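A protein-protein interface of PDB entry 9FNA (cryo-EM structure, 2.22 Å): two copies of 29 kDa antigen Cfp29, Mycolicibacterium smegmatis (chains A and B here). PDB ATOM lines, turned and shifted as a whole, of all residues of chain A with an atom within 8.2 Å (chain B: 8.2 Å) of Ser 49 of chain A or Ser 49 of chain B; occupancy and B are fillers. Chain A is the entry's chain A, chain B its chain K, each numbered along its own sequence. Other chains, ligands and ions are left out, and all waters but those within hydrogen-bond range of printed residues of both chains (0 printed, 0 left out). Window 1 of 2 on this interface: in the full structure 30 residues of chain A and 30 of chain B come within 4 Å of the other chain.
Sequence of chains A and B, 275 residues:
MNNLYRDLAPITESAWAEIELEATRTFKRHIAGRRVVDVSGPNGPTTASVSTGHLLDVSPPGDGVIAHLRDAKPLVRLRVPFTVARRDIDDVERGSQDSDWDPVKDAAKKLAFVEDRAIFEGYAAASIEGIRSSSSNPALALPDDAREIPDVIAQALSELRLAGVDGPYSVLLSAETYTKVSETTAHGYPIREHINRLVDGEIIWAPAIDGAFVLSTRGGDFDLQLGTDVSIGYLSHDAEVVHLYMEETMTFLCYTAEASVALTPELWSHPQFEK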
ATOM      1  N   ASN A  43      23.515  -2.570   7.141  1.00  0.00           N
ATOM      2  CA  ASN A  43      24.321  -1.558   7.807  1.00  0.00           C
ATOM      3  C   ASN A  43      23.668  -1.023   9.074  1.00  0.00           C
ATOM      4  O   ASN A  43      24.232  -0.133   9.716  1.00  0.00           O
ATOM      5  CB  ASN A  43      24.613  -0.403   6.844  1.00  0.00           C
ATOM      6  CG  ASN A  43      25.345  -0.859   5.596  1.00  0.00           C
ATOM      7  OD1 ASN A  43      26.491  -1.303   5.663  1.00  0.00           O
ATOM      8  ND2 ASN A  43      24.687  -0.748   4.448  1.00  0.00           N
ATOM      9  N   PRO A  45      19.750  -0.246  11.471  1.00  0.00           N
ATOM     10  CA  PRO A  45      18.541   0.582  11.340  1.00  0.00           C
ATOM     11  C   PRO A  45      18.835   2.064  11.199  1.00  0.00           C
ATOM     12  O   PRO A  45      17.974   2.806  10.712  1.00  0.00           O
ATOM     13  CB  PRO A  45      17.768   0.282  12.630  1.00  0.00           C
ATOM     14  CG  PRO A  45      18.801  -0.169  13.600  1.00  0.00           C
ATOM     15  CD  PRO A  45      19.851  -0.876  12.798  1.00  0.00           C
ATOM     16  N   THR A  46      20.017   2.520  11.611  1.00  0.00           N
ATOM     17  CA  THR A  46      20.379   3.926  11.489  1.00  0.00           C
ATOM     18  C   THR A  46      20.659   4.342  10.051  1.00  0.00           C
ATOM     19  O   THR A  46      20.701   5.544   9.770  1.00  0.00           O
ATOM     20  CB  THR A  46      21.611   4.228  12.345  1.00  0.00           C
ATOM     21  OG1 THR A  46      22.674   3.335  11.991  1.00  0.00           O
ATOM     22  CG2 THR A  46      21.287   4.068  13.820  1.00  0.00           C
ATOM     23  N   THR A  47      20.848   3.390   9.143  1.00  0.00           N
ATOM     24  CA  THR A  47      21.164   3.707   7.758  1.00  0.00           C
ATOM     25  C   THR A  47      19.907   4.164   7.029  1.00  0.00           C
ATOM     26  O   THR A  47      18.865   3.507   7.097  1.00  0.00           O
ATOM     27  CB  THR A  47      21.770   2.490   7.060  1.00  0.00           C
ATOM     28  OG1 THR A  47      22.903   2.025   7.803  1.00  0.00           O
ATOM     29  CG2 THR A  47      22.206   2.845   5.650  1.00  0.00           C
ATOM     30  N   ALA A  48      20.010   5.297   6.329  1.00  0.00           N
ATOM     31  CA  ALA A  48      18.874   5.889   5.641  1.00  0.00           C
ATOM     32  C   ALA A  48      19.126   6.212   4.176  1.00  0.00           C
ATOM     33  O   ALA A  48      18.156   6.346   3.424  1.00  0.00           O
ATOM     34  CB  ALA A  48      18.435   7.181   6.348  1.00  0.00           C
ATOM     35  N   SER A  49      20.378   6.344   3.750  1.00  0.00           N
ATOM     36  CA  SER A  49      20.669   6.736   2.378  1.00  0.00           C
ATOM     37  C   SER A  49      22.044   6.213   1.993  1.00  0.00           C
ATOM     38  O   SER A  49      22.853   5.836   2.844  1.00  0.00           O
ATOM     39  CB  SER A  49      20.599   8.256   2.209  1.00  0.00           C
ATOM     40  OG  SER A  49      21.488   8.907   3.098  1.00  0.00           O
ATOM     41  N   VAL A  50      22.296   6.196   0.686  1.00  0.00           N
ATOM     42  CA  VAL A  50      23.566   5.757   0.121  1.00  0.00           C
ATOM     43  C   VAL A  50      24.148   6.900  -0.697  1.00  0.00           C
ATOM     44  O   VAL A  50      23.510   7.377  -1.640  1.00  0.00           O
ATOM     45  CB  VAL A  50      23.397   4.501  -0.753  1.00  0.00           C
ATOM     46  CG1 VAL A  50      24.733   4.092  -1.358  1.00  0.00           C
ATOM     47  CG2 VAL A  50      22.790   3.364   0.059  1.00  0.00           C
ATOM     48  N   SER A  51      25.354   7.331  -0.343  1.00  0.00           N
ATOM     49  CA  SER A  51      26.011   8.414  -1.062  1.00  0.00           C
ATOM     50  C   SER A  51      26.382   7.956  -2.466  1.00  0.00           C
ATOM     51  O   SER A  51      26.753   6.796  -2.670  1.00  0.00           O
ATOM     52  CB  SER A  51      27.260   8.871  -0.310  1.00  0.00           C
ATOM     53  OG  SER A  51      28.003   9.806  -1.072  1.00  0.00           O
ATOM     54  N   THR A  52      26.283   8.867  -3.437  1.00  0.00           N
ATOM     55  CA  THR A  52      26.720   8.577  -4.795  1.00  0.00           C
ATOM     56  C   THR A  52      28.047   9.232  -5.145  1.00  0.00           C
ATOM     57  O   THR A  52      28.634   8.891  -6.178  1.00  0.00           O
ATOM     58  CB  THR A  52      25.665   9.036  -5.809  1.00  0.00           C
ATOM     59  OG1 THR A  52      25.497  10.455  -5.718  1.00  0.00           O
ATOM     60  CG2 THR A  52      24.335   8.354  -5.547  1.00  0.00           C
ATOM     61  N   ARG A  70      25.626  17.416  -1.769  1.00  0.00           N
ATOM     62  CA  ARG A  70      25.993  16.019  -1.939  1.00  0.00           C
ATOM     63  C   ARG A  70      24.761  15.201  -2.302  1.00  0.00           C
ATOM     64  O   ARG A  70      23.659  15.456  -1.808  1.00  0.00           O
ATOM     65  CB  ARG A  70      26.632  15.474  -0.662  1.00  0.00           C
ATOM     66  CG  ARG A  70      28.033  16.003  -0.397  1.00  0.00           C
ATOM     67  CD  ARG A  70      29.052  15.449  -1.381  1.00  0.00           C
ATOM     68  NE  ARG A  70      29.184  14.000  -1.282  1.00  0.00           N
ATOM     69  CZ  ARG A  70      30.132  13.373  -0.598  1.00  0.00           C
ATOM     70  NH1 ARG A  70      31.060  14.035   0.073  1.00  0.00           N
ATOM     71  NH2 ARG A  70      30.148  12.043  -0.585  1.00  0.00           N
ATOM     72  N   ASP A  71      24.954  14.211  -3.170  1.00  0.00           N
ATOM     73  CA  ASP A  71      23.854  13.438  -3.727  1.00  0.00           C
ATOM     74  C   ASP A  71      23.776  12.063  -3.075  1.00  0.00           C
ATOM     75  O   ASP A  71      24.781  11.350  -2.967  1.00  0.00           O
ATOM     76  CB  ASP A  71      24.012  13.292  -5.241  1.00  0.00           C
ATOM     77  CG  ASP A  71      22.729  12.865  -5.922  1.00  0.00           C
ATOM     78  OD1 ASP A  71      21.649  13.346  -5.519  1.00  0.00           O
ATOM     79  OD2 ASP A  71      22.799  12.049  -6.865  1.00  0.00           O
ATOM     80  N   ALA A  72      22.570  11.694  -2.651  1.00  0.00           N
ATOM     81  CA  ALA A  72      22.348  10.427  -1.976  1.00  0.00           C
ATOM     82  C   ALA A  72      21.049   9.812  -2.474  1.00  0.00           C
ATOM     83  O   ALA A  72      20.130  10.510  -2.911  1.00  0.00           O
ATOM     84  CB  ALA A  72      22.306  10.601  -0.454  1.00  0.00           C
ATOM     85  N   LYS A  73      20.992   8.485  -2.400  1.00  0.00           N
ATOM     86  CA  LYS A  73      19.825   7.707  -2.779  1.00  0.00           C
ATOM     87  C   LYS A  73      19.123   7.239  -1.515  1.00  0.00           C
ATOM     88  O   LYS A  73      19.751   6.548  -0.698  1.00  0.00           O
ATOM     89  CB  LYS A  73      20.233   6.509  -3.633  1.00  0.00           C
ATOM     90  CG  LYS A  73      21.077   6.858  -4.851  1.00  0.00           C
ATOM     91  CD  LYS A  73      20.423   7.912  -5.731  1.00  0.00           C
ATOM     92  CE  LYS A  73      19.038   7.482  -6.177  1.00  0.00           C
ATOM     93  NZ  LYS A  73      18.710   8.000  -7.532  1.00  0.00           N
ATOM     94  N   PRO A  74      17.861   7.597  -1.288  1.00  0.00           N
ATOM     95  CA  PRO A  74      17.177   7.163  -0.067  1.00  0.00           C
ATOM     96  C   PRO A  74      16.818   5.685  -0.117  1.00  0.00           C
ATOM     97  O   PRO A  74      16.695   5.070  -1.178  1.00  0.00           O
ATOM     98  CB  PRO A  74      15.927   8.043  -0.034  1.00  0.00           C
ATOM     99  CG  PRO A  74      15.647   8.324  -1.463  1.00  0.00           C
ATOM    100  CD  PRO A  74      16.992   8.446  -2.123  1.00  0.00           C
ATOM    101  N   LEU A  75      16.647   5.118   1.072  1.00  0.00           N
ATOM    102  CA  LEU A  75      16.221   3.737   1.239  1.00  0.00           C
ATOM    103  C   LEU A  75      14.716   3.690   1.466  1.00  0.00           C
ATOM    104  O   LEU A  75      14.141   4.582   2.096  1.00  0.00           O
ATOM    105  CB  LEU A  75      16.944   3.085   2.417  1.00  0.00           C
ATOM    106  CG  LEU A  75      18.165   2.233   2.073  1.00  0.00           C
ATOM    107  CD1 LEU A  75      19.265   3.092   1.482  1.00  0.00           C
ATOM    108  CD2 LEU A  75      18.665   1.499   3.303  1.00  0.00           C
ATOM    109  N   VAL A  76      14.078   2.642   0.952  1.00  0.00           N
ATOM    110  CA  VAL A  76      12.632   2.480   1.042  1.00  0.00           C
ATOM    111  C   VAL A  76      12.342   1.229   1.859  1.00  0.00           C
ATOM    112  O   VAL A  76      13.011   0.201   1.695  1.00  0.00           O
ATOM    113  CB  VAL A  76      11.981   2.394  -0.350  1.00  0.00           C
ATOM    114  CG1 VAL A  76      12.562   1.241  -1.152  1.00  0.00           C
ATOM    115  CG2 VAL A  76      10.472   2.267  -0.225  1.00  0.00           C
ATOM    116  N   GLN A 225      21.534  -2.489  -1.897  1.00  0.00           N
ATOM    117  CA  GLN A 225      21.867  -1.983  -0.575  1.00  0.00           C
ATOM    118  C   GLN A 225      20.726  -2.286   0.387  1.00  0.00           C
ATOM    119  O   GLN A 225      19.572  -1.944   0.115  1.00  0.00           O
ATOM    120  CB  GLN A 225      22.130  -0.478  -0.627  1.00  0.00           C
ATOM    121  CG  GLN A 225      23.443  -0.101  -1.285  1.00  0.00           C
ATOM    122  CD  GLN A 225      24.639  -0.352  -0.390  1.00  0.00           C
ATOM    123  OE1 GLN A 225      24.509  -0.437   0.831  1.00  0.00           O
ATOM    124  NE2 GLN A 225      25.813  -0.470  -0.996  1.00  0.00           N
ATOM    125  N   GLY A 227      19.434  -1.916   4.432  1.00  0.00           N
ATOM    126  CA  GLY A 227      19.609  -1.366   5.761  1.00  0.00           C
ATOM    127  C   GLY A 227      19.359  -2.438   6.799  1.00  0.00           C
ATOM    128  O   GLY A 227      20.168  -2.647   7.708  1.00  0.00           O
ATOM    129  N   THR A 249      14.176  -3.074   4.412  1.00  0.00           N
ATOM    130  CA  THR A 249      14.557  -1.737   3.972  1.00  0.00           C
ATOM    131  C   THR A 249      15.703  -1.842   2.974  1.00  0.00           C
ATOM    132  O   THR A 249      16.778  -2.351   3.310  1.00  0.00           O
ATOM    133  CB  THR A 249      14.973  -0.871   5.163  1.00  0.00           C
ATOM    134  OG1 THR A 249      14.086  -1.107   6.263  1.00  0.00           O
ATOM    135  CG2 THR A 249      14.936   0.601   4.797  1.00  0.00           C
ATOM    136  N   THR A 251      17.418  -0.521  -1.220  1.00  0.00           N
ATOM    137  CA  THR A 251      17.465   0.259  -2.449  1.00  0.00           C
ATOM    138  C   THR A 251      18.372  -0.480  -3.425  1.00  0.00           C
ATOM    139  O   THR A 251      19.117  -1.382  -3.038  1.00  0.00           O
ATOM    140  CB  THR A 251      17.963   1.691  -2.211  1.00  0.00           C
ATOM    141  OG1 THR A 251      17.885   2.435  -3.433  1.00  0.00           O
ATOM    142  CG2 THR A 251      19.398   1.693  -1.715  1.00  0.00           C
ATOM    143  N   LEU A 253      20.986  -0.009  -7.010  1.00  0.00           N
ATOM    144  CA  LEU A 253      21.772   0.866  -7.864  1.00  0.00           C
ATOM    145  C   LEU A 253      22.404   0.066  -8.997  1.00  0.00           C
ATOM    146  O   LEU A 253      22.914  -1.040  -8.783  1.00  0.00           O
ATOM    147  CB  LEU A 253      22.868   1.575  -7.064  1.00  0.00           C
ATOM    148  CG  LEU A 253      22.393   2.420  -5.882  1.00  0.00           C
ATOM    149  CD1 LEU A 253      22.635   1.689  -4.573  1.00  0.00           C
ATOM    150  CD2 LEU A 253      23.086   3.769  -5.876  1.00  0.00           C
ATOM    151  N   ASN B  43      33.264  12.617   9.412  1.00  0.00           N
ATOM    152  CA  ASN B  43      32.970  11.218   9.145  1.00  0.00           C
ATOM    153  C   ASN B  43      33.557  10.733   7.827  1.00  0.00           C
ATOM    154  O   ASN B  43      33.349   9.573   7.461  1.00  0.00           O
ATOM    155  CB  ASN B  43      31.455  10.991   9.155  1.00  0.00           C
ATOM    156  CG  ASN B  43      30.820  11.373  10.479  1.00  0.00           C
ATOM    157  OD1 ASN B  43      31.081  10.750  11.508  1.00  0.00           O
ATOM    158  ND2 ASN B  43      29.978  12.400  10.459  1.00  0.00           N
ATOM    159  N   PRO B  45      35.054  11.793   3.544  1.00  0.00           N
ATOM    160  CA  PRO B  45      34.485  12.312   2.291  1.00  0.00           C
ATOM    161  C   PRO B  45      33.329  11.484   1.761  1.00  0.00           C
ATOM    162  O   PRO B  45      32.537  11.996   0.960  1.00  0.00           O
ATOM    163  CB  PRO B  45      35.678  12.294   1.328  1.00  0.00           C
ATOM    164  CG  PRO B  45      36.599  11.263   1.879  1.00  0.00           C
ATOM    165  CD  PRO B  45      36.431  11.302   3.367  1.00  0.00           C
ATOM    166  N   THR B  46      33.208  10.224   2.175  1.00  0.00           N
ATOM    167  CA  THR B  46      32.113   9.373   1.727  1.00  0.00           C
ATOM    168  C   THR B  46      30.773   9.761   2.340  1.00  0.00           C
ATOM    169  O   THR B  46      29.733   9.315   1.843  1.00  0.00           O
ATOM    170  CB  THR B  46      32.411   7.911   2.062  1.00  0.00           C
ATOM    171  OG1 THR B  46      32.691   7.785   3.461  1.00  0.00           O
ATOM    172  CG2 THR B  46      33.603   7.413   1.262  1.00  0.00           C
ATOM    173  N   THR B  47      30.772  10.571   3.394  1.00  0.00           N
ATOM    174  CA  THR B  47      29.536  10.951   4.063  1.00  0.00           C
ATOM    175  C   THR B  47      28.802  12.004   3.241  1.00  0.00           C
ATOM    176  O   THR B  47      29.395  13.002   2.823  1.00  0.00           O
ATOM    177  CB  THR B  47      29.834  11.483   5.463  1.00  0.00           C
ATOM    178  OG1 THR B  47      30.594  10.513   6.194  1.00  0.00           O
ATOM    179  CG2 THR B  47      28.545  11.775   6.210  1.00  0.00           C
ATOM    180  N   ALA B  48      27.507  11.775   3.013  1.00  0.00           N
ATOM    181  CA  ALA B  48      26.698  12.658   2.187  1.00  0.00           C
ATOM    182  C   ALA B  48      25.407  13.123   2.842  1.00  0.00           C
ATOM    183  O   ALA B  48      24.858  14.142   2.411  1.00  0.00           O
ATOM    184  CB  ALA B  48      26.341  11.971   0.859  1.00  0.00           C
ATOM    185  N   SER B  49      24.907  12.421   3.854  1.00  0.00           N
ATOM    186  CA  SER B  49      23.631  12.777   4.459  1.00  0.00           C
ATOM    187  C   SER B  49      23.605  12.276   5.895  1.00  0.00           C
ATOM    188  O   SER B  49      24.407  11.431   6.298  1.00  0.00           O
ATOM    189  CB  SER B  49      22.459  12.198   3.661  1.00  0.00           C
ATOM    190  OG  SER B  49      22.567  10.791   3.548  1.00  0.00           O
ATOM    191  N   VAL B  50      22.663  12.816   6.664  1.00  0.00           N
ATOM    192  CA  VAL B  50      22.460  12.446   8.060  1.00  0.00           C
ATOM    193  C   VAL B  50      21.032  11.945   8.219  1.00  0.00           C
ATOM    194  O   VAL B  50      20.080  12.673   7.925  1.00  0.00           O
ATOM    195  CB  VAL B  50      22.723  13.631   9.007  1.00  0.00           C
ATOM    196  CG1 VAL B  50      22.463  13.223  10.450  1.00  0.00           C
ATOM    197  CG2 VAL B  50      24.143  14.152   8.828  1.00  0.00           C
ATOM    198  N   SER B  51      20.885  10.711   8.690  1.00  0.00           N
ATOM    199  CA  SER B  51      19.563  10.131   8.892  1.00  0.00           C
ATOM    200  C   SER B  51      18.849  10.850  10.028  1.00  0.00           C
ATOM    201  O   SER B  51      19.480  11.250  11.012  1.00  0.00           O
ATOM    202  CB  SER B  51      19.679   8.640   9.202  1.00  0.00           C
ATOM    203  OG  SER B  51      18.424   8.093   9.565  1.00  0.00           O
ATOM    204  N   THR B  52      17.531  11.014   9.895  1.00  0.00           N
ATOM    205  CA  THR B  52      16.727  11.582  10.968  1.00  0.00           C
ATOM    206  C   THR B  52      15.911  10.539  11.716  1.00  0.00           C
ATOM    207  O   THR B  52      15.362  10.851  12.778  1.00  0.00           O
ATOM    208  CB  THR B  52      15.771  12.648  10.416  1.00  0.00           C
ATOM    209  OG1 THR B  52      14.864  12.044   9.488  1.00  0.00           O
ATOM    210  CG2 THR B  52      16.543  13.753   9.720  1.00  0.00           C
ATOM    211  N   ARG B  70      12.832   6.527   4.057  1.00  0.00           N
ATOM    212  CA  ARG B  70      13.651   7.024   5.151  1.00  0.00           C
ATOM    213  C   ARG B  70      14.064   8.464   4.876  1.00  0.00           C
ATOM    214  O   ARG B  70      14.331   8.841   3.732  1.00  0.00           O
ATOM    215  CB  ARG B  70      14.889   6.146   5.335  1.00  0.00           C
ATOM    216  CG  ARG B  70      14.594   4.778   5.932  1.00  0.00           C
ATOM    217  CD  ARG B  70      14.192   4.864   7.395  1.00  0.00           C
ATOM    218  NE  ARG B  70      15.259   5.403   8.231  1.00  0.00           N
ATOM    219  CZ  ARG B  70      16.105   4.670   8.943  1.00  0.00           C
ATOM    220  NH1 ARG B  70      16.046   3.349   8.949  1.00  0.00           N
ATOM    221  NH2 ARG B  70      17.037   5.281   9.669  1.00  0.00           N
ATOM    222  N   ASP B  71      14.116   9.267   5.935  1.00  0.00           N
ATOM    223  CA  ASP B  71      14.348  10.699   5.815  1.00  0.00           C
ATOM    224  C   ASP B  71      15.776  11.050   6.215  1.00  0.00           C
ATOM    225  O   ASP B  71      16.265  10.630   7.270  1.00  0.00           O
ATOM    226  CB  ASP B  71      13.356  11.477   6.680  1.00  0.00           C
ATOM    227  CG  ASP B  71      13.273  12.941   6.298  1.00  0.00           C
ATOM    228  OD1 ASP B  71      13.316  13.245   5.088  1.00  0.00           O
ATOM    229  OD2 ASP B  71      13.161  13.788   7.208  1.00  0.00           O
ATOM    230  N   ALA B  72      16.435  11.834   5.365  1.00  0.00           N
ATOM    231  CA  ALA B  72      17.816  12.222   5.593  1.00  0.00           C
ATOM    232  C   ALA B  72      17.996  13.685   5.219  1.00  0.00           C
ATOM    233  O   ALA B  72      17.276  14.231   4.380  1.00  0.00           O
ATOM    234  CB  ALA B  72      18.785  11.345   4.792  1.00  0.00           C
ATOM    235  N   LYS B  73      18.976  14.311   5.865  1.00  0.00           N
ATOM    236  CA  LYS B  73      19.344  15.696   5.621  1.00  0.00           C
ATOM    237  C   LYS B  73      20.630  15.721   4.811  1.00  0.00           C
ATOM    238  O   LYS B  73      21.642  15.169   5.271  1.00  0.00           O
ATOM    239  CB  LYS B  73      19.534  16.441   6.941  1.00  0.00           C
ATOM    240  CG  LYS B  73      18.351  16.348   7.894  1.00  0.00           C
ATOM    241  CD  LYS B  73      17.045  16.782   7.248  1.00  0.00           C
ATOM    242  CE  LYS B  73      17.141  18.189   6.690  1.00  0.00           C
ATOM    243  NZ  LYS B  73      15.841  18.906   6.778  1.00  0.00           N
ATOM    244  N   PRO B  74      20.648  16.307   3.616  1.00  0.00           N
ATOM    245  CA  PRO B  74      21.879  16.326   2.821  1.00  0.00           C
ATOM    246  C   PRO B  74      22.901  17.301   3.387  1.00  0.00           C
ATOM    247  O   PRO B  74      22.580  18.253   4.102  1.00  0.00           O
ATOM    248  CB  PRO B  74      21.395  16.761   1.437  1.00  0.00           C
ATOM    249  CG  PRO B  74      20.202  17.597   1.720  1.00  0.00           C
ATOM    250  CD  PRO B  74      19.534  16.962   2.907  1.00  0.00           C
ATOM    251  N   LEU B  75      24.158  17.045   3.044  1.00  0.00           N
ATOM    252  CA  LEU B  75      25.272  17.904   3.412  1.00  0.00           C
ATOM    253  C   LEU B  75      25.592  18.849   2.262  1.00  0.00           C
ATOM    254  O   LEU B  75      25.470  18.486   1.090  1.00  0.00           O
ATOM    255  CB  LEU B  75      26.508  17.071   3.759  1.00  0.00           C
ATOM    256  CG  LEU B  75      26.752  16.811   5.244  1.00  0.00           C
ATOM    257  CD1 LEU B  75      25.641  15.960   5.827  1.00  0.00           C
ATOM    258  CD2 LEU B  75      28.099  16.145   5.452  1.00  0.00           C
ATOM    259  N   VAL B  76      26.007  20.067   2.603  1.00  0.00           N
ATOM    260  CA  VAL B  76      26.305  21.100   1.620  1.00  0.00           C
ATOM    261  C   VAL B  76      27.782  21.450   1.726  1.00  0.00           C
ATOM    262  O   VAL B  76      28.324  21.560   2.833  1.00  0.00           O
ATOM    263  CB  VAL B  76      25.425  22.346   1.819  1.00  0.00           C
ATOM    264  CG1 VAL B  76      25.605  22.922   3.214  1.00  0.00           C
ATOM    265  CG2 VAL B  76      25.727  23.388   0.755  1.00  0.00           C
ATOM    266  N   GLN B 225      26.921  18.849  11.969  1.00  0.00           N
ATOM    267  CA  GLN B 225      27.486  17.663  11.347  1.00  0.00           C
ATOM    268  C   GLN B 225      28.477  18.079  10.268  1.00  0.00           C
ATOM    269  O   GLN B 225      28.141  18.868   9.379  1.00  0.00           O
ATOM    270  CB  GLN B 225      26.380  16.798  10.742  1.00  0.00           C
ATOM    271  CG  GLN B 225      25.539  16.062  11.768  1.00  0.00           C
ATOM    272  CD  GLN B 225      26.252  14.866  12.359  1.00  0.00           C
ATOM    273  OE1 GLN B 225      27.194  14.334  11.770  1.00  0.00           O
ATOM    274  NE2 GLN B 225      25.806  14.432  13.531  1.00  0.00           N
ATOM    275  N   GLY B 227      31.216  16.612   7.349  1.00  0.00           N
ATOM    276  CA  GLY B 227      31.768  15.512   6.586  1.00  0.00           C
ATOM    277  C   GLY B 227      33.274  15.630   6.526  1.00  0.00           C
ATOM    278  O   GLY B 227      34.001  14.674   6.814  1.00  0.00           O
ATOM    279  N   THR B 249      32.444  20.827   4.231  1.00  0.00           N
ATOM    280  CA  THR B 249      31.168  20.169   3.975  1.00  0.00           C
ATOM    281  C   THR B 249      30.433  19.961   5.293  1.00  0.00           C
ATOM    282  O   THR B 249      30.938  19.272   6.187  1.00  0.00           O
ATOM    283  CB  THR B 249      31.383  18.825   3.274  1.00  0.00           C
ATOM    284  OG1 THR B 249      32.404  18.958   2.280  1.00  0.00           O
ATOM    285  CG2 THR B 249      30.100  18.353   2.613  1.00  0.00           C
ATOM    286  N   THR B 251      26.379  20.414   7.665  1.00  0.00           N
ATOM    287  CA  THR B 251      24.955  20.679   7.822  1.00  0.00           C
ATOM    288  C   THR B 251      24.696  20.926   9.303  1.00  0.00           C
ATOM    289  O   THR B 251      25.538  20.625  10.152  1.00  0.00           O
ATOM    290  CB  THR B 251      24.088  19.528   7.297  1.00  0.00           C
ATOM    291  OG1 THR B 251      22.704  19.892   7.380  1.00  0.00           O
ATOM    292  CG2 THR B 251      24.320  18.260   8.099  1.00  0.00           C
ATOM    293  N   LEU B 253      21.593  20.827  12.507  1.00  0.00           N
ATOM    294  CA  LEU B 253      20.309  20.330  12.974  1.00  0.00           C
ATOM    295  C   LEU B 253      20.004  20.881  14.360  1.00  0.00           C
ATOM    296  O   LEU B 253      20.884  20.933  15.228  1.00  0.00           O
ATOM    297  CB  LEU B 253      20.295  18.799  13.016  1.00  0.00           C
ATOM    298  CG  LEU B 253      20.592  18.090  11.695  1.00  0.00           C
ATOM    299  CD1 LEU B 253      22.015  17.558  11.683  1.00  0.00           C
ATOM    300  CD2 LEU B 253      19.600  16.967  11.456  1.00  0.00           C
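The side-chain hydroxyl of Ser 51 of chain A sits close to the backbone carbonyl oxygen of Thr 46 of chain B (3.4 Å). O of Leu 75 of chain B is in hydrogen-bond range of N of Arg 70 of chain A (3.1 Å). The backbone NH (N) of Arg 70 of chain B lies within hydrogen-bond range of the backbone carbonyl oxygen (O) of Leu 75 of chain A, 3.1 Å away. NH1 of Arg 70 of chain B sits at hydrogen-bond distance from O of Pro 45 of chain A, at 2.7 Å. NH1 of Arg 70 of chain A lies within hydrogen-bond range of O of Thr 47 of chain B (3.4 Å). O of Thr 47 of chain A lies within hydrogen-bond range of NH1 of Arg 70 of chain B (3.4 Å). OG of Ser 49 of chain A sits close to OG of Ser 49 of chain B (2.2 Å). The backbone carbonyl oxygen of Thr 46 of chain A lies close to the side-chain hydroxyl of Ser 51 of chain B, 3.4 Å away. The guanidinium group (NH1) of Arg 70 of chain A is in hydrogen-bond range of the backbone carbonyl oxygen (O) of Pro 45 of chain B, at 2.7 Å.
The backbone NH (N) of Leu 75 of chain B is in hydrogen-bond range of the backbone carbonyl oxygen (O) of Ala 48 of chain B, 3.1 Å away. OG1 of Thr 47 of chain B sits close to O of Asn 43 of chain B (3.2 Å). OG of Ser 51 of chain B lies within hydrogen-bond range of NH2 of Arg 70 of chain B, 3.1 Å away.
Among the printed residues, merely in contact across the chains: Thr 46 of chain A with Arg 70 of chain B, Ala 48 of chain A with Ser 51 of chain B, Ala 48 of chain A with Arg 70 of chain B, Ser 51 of chain A with Ala 48 of chain B, Arg 70 of chain A with Thr 46 of chain B and Arg 70 of chain A with Ala 48 of chain B.
Of chain A, only Ser 51 and Arg 70 come within 4 Å of Ala 48 of chain B. Of the printed residues of chain A, Thr 47 of chain B touches Arg 70 (3.4 Å). Of the printed residues of chain A, Arg 70 of chain B touches Pro 45, Thr 46, Thr 47, Ala 48 and Leu 75. Of the printed residues of chain B, Pro 45 of chain A touches Arg 70. Printed residues of chain A within 4 Å of Pro 45 of chain B: Arg 70 (2.7 Å). The nearest printed residue of chain B that does not touch Ser 49 of chain A is Ala 72 of chain B (4.01 Å). The nearest printed residue of chain A that does not touch Ser 49 of chain B is Ala 72 of chain A (4.02 Å). The nearest printed residue of chain A that does not touch Ser 51 of chain B is Thr 47 of chain A (4.9 Å).
Of the 21 printed residues of chain A, 8 touch a printed residue of chain B. Printed residues of chain B that touch a printed residue of chain A: Pro 45, Thr 46, Thr 47, Ala 48, Ser 49, Ser 51, Arg 70 and Leu 75. Hydrophobic or aromatic side chains of chain B that line the printed part of chain A: Ala 48. Among the printed residues, 15 pairs touch across the chains. Among the printed residues, no Asp or Glu carboxylate lies within 4 Å of a Lys or Arg side-chain nitrogen of the other chain.
Pro 45 of chain A touches Arg 70 of chain B, and with the chains exchanged Arg 70 of chain A touches Pro 45 of chain B. Ala 48 of chain A touches Arg 70 of chain B, and with the chains exchanged Arg 70 of chain A touches Ala 48 of chain B.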
